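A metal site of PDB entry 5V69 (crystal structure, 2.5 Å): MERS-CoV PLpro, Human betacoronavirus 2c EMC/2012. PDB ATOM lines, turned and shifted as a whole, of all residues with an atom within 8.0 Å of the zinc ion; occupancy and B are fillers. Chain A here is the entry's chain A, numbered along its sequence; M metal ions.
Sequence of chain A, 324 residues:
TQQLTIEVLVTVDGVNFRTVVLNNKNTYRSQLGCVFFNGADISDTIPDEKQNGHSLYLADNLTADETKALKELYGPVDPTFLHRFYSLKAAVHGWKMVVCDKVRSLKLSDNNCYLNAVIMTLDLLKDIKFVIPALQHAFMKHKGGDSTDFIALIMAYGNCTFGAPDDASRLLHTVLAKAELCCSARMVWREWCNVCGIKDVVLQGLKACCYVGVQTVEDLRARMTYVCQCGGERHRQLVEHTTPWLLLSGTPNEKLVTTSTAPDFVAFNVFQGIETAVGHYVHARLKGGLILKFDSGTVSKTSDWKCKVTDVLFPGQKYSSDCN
Of the 14 residues printed, 4 come within 4 Å of the zinc ion.
The nearest printed residue that does not touch the zinc ion is Val 195 (4.1 Å).
The side-chain sulfur of Cys 230 lies close to the backbone NH of Gly 232.
SG of Cys 193 lies close to N of Val 195 (3.2 Å).
NH1 of Arg 234 sits close to SG of Cys 228, at 3.4 Å.
The zinc ion is bound by the side-chain sulfur of Cys 230, the side-chain sulfur of Cys 196, the side-chain sulfur of Cys 193 and the side-chain sulfur of Cys 228.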
ATOM      1  N   TRP A 192      -0.384 -11.319   4.096  1.00  0.00           N
ATOM      2  CA  TRP A 192       0.132 -12.197   3.059  1.00  0.00           C
ATOM      3  C   TRP A 192      -0.867 -13.305   2.751  1.00  0.00           C
ATOM      4  O   TRP A 192      -1.539 -13.812   3.651  1.00  0.00           O
ATOM      5  CB  TRP A 192       1.499 -12.789   3.443  1.00  0.00           C
ATOM      6  CG  TRP A 192       1.467 -13.712   4.608  1.00  0.00           C
ATOM      7  CD1 TRP A 192       1.336 -15.075   4.570  1.00  0.00           C
ATOM      8  CD2 TRP A 192       1.575 -13.365   5.995  1.00  0.00           C
ATOM      9  NE1 TRP A 192       1.351 -15.591   5.849  1.00  0.00           N
ATOM     10  CE2 TRP A 192       1.503 -14.556   6.740  1.00  0.00           C
ATOM     11  CE3 TRP A 192       1.738 -12.153   6.671  1.00  0.00           C
ATOM     12  CZ2 TRP A 192       1.579 -14.577   8.124  1.00  0.00           C
ATOM     13  CZ3 TRP A 192       1.814 -12.173   8.055  1.00  0.00           C
ATOM     14  CH2 TRP A 192       1.732 -13.373   8.765  1.00  0.00           C
ATOM     15  N   CYS A 193      -0.938 -13.660   1.471  1.00  0.00           N
ATOM     16  CA  CYS A 193      -1.704 -14.795   0.981  1.00  0.00           C
ATOM     17  C   CYS A 193      -0.805 -15.623   0.072  1.00  0.00           C
ATOM     18  O   CYS A 193       0.030 -15.077  -0.648  1.00  0.00           O
ATOM     19  CB  CYS A 193      -2.951 -14.336   0.216  1.00  0.00           C
ATOM     20  SG  CYS A 193      -3.533 -15.500  -1.035  1.00  0.00           S
ATOM     21  N   ASN A 194      -0.972 -16.946   0.112  1.00  0.00           N
ATOM     22  CA  ASN A 194      -0.075 -17.822  -0.642  1.00  0.00           C
ATOM     23  C   ASN A 194      -0.188 -17.592  -2.148  1.00  0.00           C
ATOM     24  O   ASN A 194       0.781 -17.817  -2.884  1.00  0.00           O
ATOM     25  CB  ASN A 194      -0.365 -19.284  -0.308  1.00  0.00           C
ATOM     26  CG  ASN A 194       0.168 -19.683   1.048  1.00  0.00           C
ATOM     27  OD1 ASN A 194       1.123 -19.098   1.564  1.00  0.00           O
ATOM     28  ND2 ASN A 194      -0.449 -20.692   1.644  1.00  0.00           N
ATOM     29  N   VAL A 195      -1.345 -17.135  -2.620  1.00  0.00           N
ATOM     30  CA  VAL A 195      -1.521 -16.873  -4.044  1.00  0.00           C
ATOM     31  C   VAL A 195      -1.003 -15.478  -4.404  1.00  0.00           C
ATOM     32  O   VAL A 195      -0.089 -15.324  -5.225  1.00  0.00           O
ATOM     33  CB  VAL A 195      -2.995 -17.036  -4.457  1.00  0.00           C
ATOM     34  CG1 VAL A 195      -3.195 -16.590  -5.893  1.00  0.00           C
ATOM     35  CG2 VAL A 195      -3.432 -18.474  -4.271  1.00  0.00           C
ATOM     36  N   CYS A 196      -1.592 -14.445  -3.792  1.00  0.00           N
ATOM     37  CA  CYS A 196      -1.267 -13.071  -4.172  1.00  0.00           C
ATOM     38  C   CYS A 196       0.124 -12.675  -3.717  1.00  0.00           C
ATOM     39  O   CYS A 196       0.910 -12.102  -4.496  1.00  0.00           O
ATOM     40  CB  CYS A 196      -2.320 -12.114  -3.602  1.00  0.00           C
ATOM     41  SG  CYS A 196      -4.027 -12.658  -3.854  1.00  0.00           S
ATOM     42  N   GLY A 197       0.461 -12.945  -2.465  1.00  0.00           N
ATOM     43  CA  GLY A 197       1.751 -12.527  -1.943  1.00  0.00           C
ATOM     44  C   GLY A 197       1.639 -11.706  -0.677  1.00  0.00           C
ATOM     45  O   GLY A 197       0.643 -11.802   0.037  1.00  0.00           O
ATOM     46  N   VAL A 227     -10.260 -14.207   4.879  1.00  0.00           N
ATOM     47  CA  VAL A 227     -10.397 -14.614   3.477  1.00  0.00           C
ATOM     48  C   VAL A 227      -9.848 -13.503   2.602  1.00  0.00           C
ATOM     49  O   VAL A 227     -10.239 -12.340   2.728  1.00  0.00           O
ATOM     50  CB  VAL A 227     -11.854 -14.931   3.132  1.00  0.00           C
ATOM     51  CG1 VAL A 227     -11.953 -15.448   1.703  1.00  0.00           C
ATOM     52  CG2 VAL A 227     -12.433 -15.942   4.112  1.00  0.00           C
ATOM     53  N   CYS A 228      -8.941 -13.864   1.690  1.00  0.00           N
ATOM     54  CA  CYS A 228      -8.372 -12.925   0.741  1.00  0.00           C
ATOM     55  C   CYS A 228      -9.370 -12.608  -0.374  1.00  0.00           C
ATOM     56  O   CYS A 228     -10.357 -13.320  -0.570  1.00  0.00           O
ATOM     57  CB  CYS A 228      -7.081 -13.489   0.141  1.00  0.00           C
ATOM     58  SG  CYS A 228      -6.298 -12.438  -1.102  1.00  0.00           S
ATOM     59  N   GLN A 229      -9.097 -11.519  -1.100  1.00  0.00           N
ATOM     60  CA  GLN A 229      -9.933 -11.182  -2.240  1.00  0.00           C
ATOM     61  C   GLN A 229      -9.942 -12.298  -3.280  1.00  0.00           C
ATOM     62  O   GLN A 229     -10.954 -12.501  -3.968  1.00  0.00           O
ATOM     63  CB  GLN A 229      -9.466  -9.880  -2.889  1.00  0.00           C
ATOM     64  CG  GLN A 229      -9.766  -8.627  -2.076  1.00  0.00           C
ATOM     65  CD  GLN A 229      -9.748  -7.371  -2.919  1.00  0.00           C
ATOM     66  OE1 GLN A 229     -10.599  -7.190  -3.789  1.00  0.00           O
ATOM     67  NE2 GLN A 229      -8.786  -6.499  -2.657  1.00  0.00           N
ATOM     68  N   CYS A 230      -8.832 -13.027  -3.408  1.00  0.00           N
ATOM     69  CA  CYS A 230      -8.792 -14.160  -4.322  1.00  0.00           C
ATOM     70  C   CYS A 230      -9.651 -15.326  -3.852  1.00  0.00           C
ATOM     71  O   CYS A 230      -9.984 -16.197  -4.652  1.00  0.00           O
ATOM     72  CB  CYS A 230      -7.344 -14.633  -4.502  1.00  0.00           C
ATOM     73  SG  CYS A 230      -6.725 -15.642  -3.134  1.00  0.00           S
ATOM     74  N   GLY A 231     -10.012 -15.353  -2.566  1.00  0.00           N
ATOM     75  CA  GLY A 231     -10.834 -16.405  -2.019  1.00  0.00           C
ATOM     76  C   GLY A 231     -10.120 -17.418  -1.151  1.00  0.00           C
ATOM     77  O   GLY A 231     -10.726 -18.418  -0.781  1.00  0.00           O
ATOM     78  N   GLY A 232      -8.857 -17.178  -0.809  1.00  0.00           N
ATOM     79  CA  GLY A 232      -8.103 -18.116   0.001  1.00  0.00           C
ATOM     80  C   GLY A 232      -7.683 -17.565   1.352  1.00  0.00           C
ATOM     81  O   GLY A 232      -8.086 -16.460   1.735  1.00  0.00           O
ATOM     82  N   GLU A 233      -6.868 -18.314   2.081  1.00  0.00           N
ATOM     83  CA  GLU A 233      -6.448 -17.930   3.422  1.00  0.00           C
ATOM     84  C   GLU A 233      -5.501 -16.731   3.344  1.00  0.00           C
ATOM     85  O   GLU A 233      -4.387 -16.844   2.829  1.00  0.00           O
ATOM     86  CB  GLU A 233      -5.772 -19.098   4.136  1.00  0.00           C
ATOM     87  CG  GLU A 233      -6.710 -19.928   4.986  1.00  0.00           C
ATOM     88  CD  GLU A 233      -5.979 -20.689   6.080  1.00  0.00           C
ATOM     89  OE1 GLU A 233      -4.758 -20.455   6.256  1.00  0.00           O
ATOM     90  OE2 GLU A 233      -6.612 -21.499   6.774  1.00  0.00           O
ATOM     91  N   ARG A 234      -5.949 -15.586   3.850  1.00  0.00           N
ATOM     92  CA  ARG A 234      -5.105 -14.425   4.014  1.00  0.00           C
ATOM     93  C   ARG A 234      -4.768 -14.247   5.488  1.00  0.00           C
ATOM     94  O   ARG A 234      -5.631 -14.372   6.353  1.00  0.00           O
ATOM     95  CB  ARG A 234      -5.788 -13.164   3.479  1.00  0.00           C
ATOM     96  CG  ARG A 234      -4.871 -11.949   3.386  1.00  0.00           C
ATOM     97  CD  ARG A 234      -5.502 -10.844   2.554  1.00  0.00           C
ATOM     98  NE  ARG A 234      -4.543  -9.782   2.248  1.00  0.00           N
ATOM     99  CZ  ARG A 234      -3.726  -9.799   1.203  1.00  0.00           C
ATOM    100  NH1 ARG A 234      -3.740 -10.822   0.356  1.00  0.00           N
ATOM    101  NH2 ARG A 234      -2.891  -8.790   0.998  1.00  0.00           N
HETATM  102 ZN    ZN M   1      -5.050 -14.203  -2.358  1.00  0.00          ZN
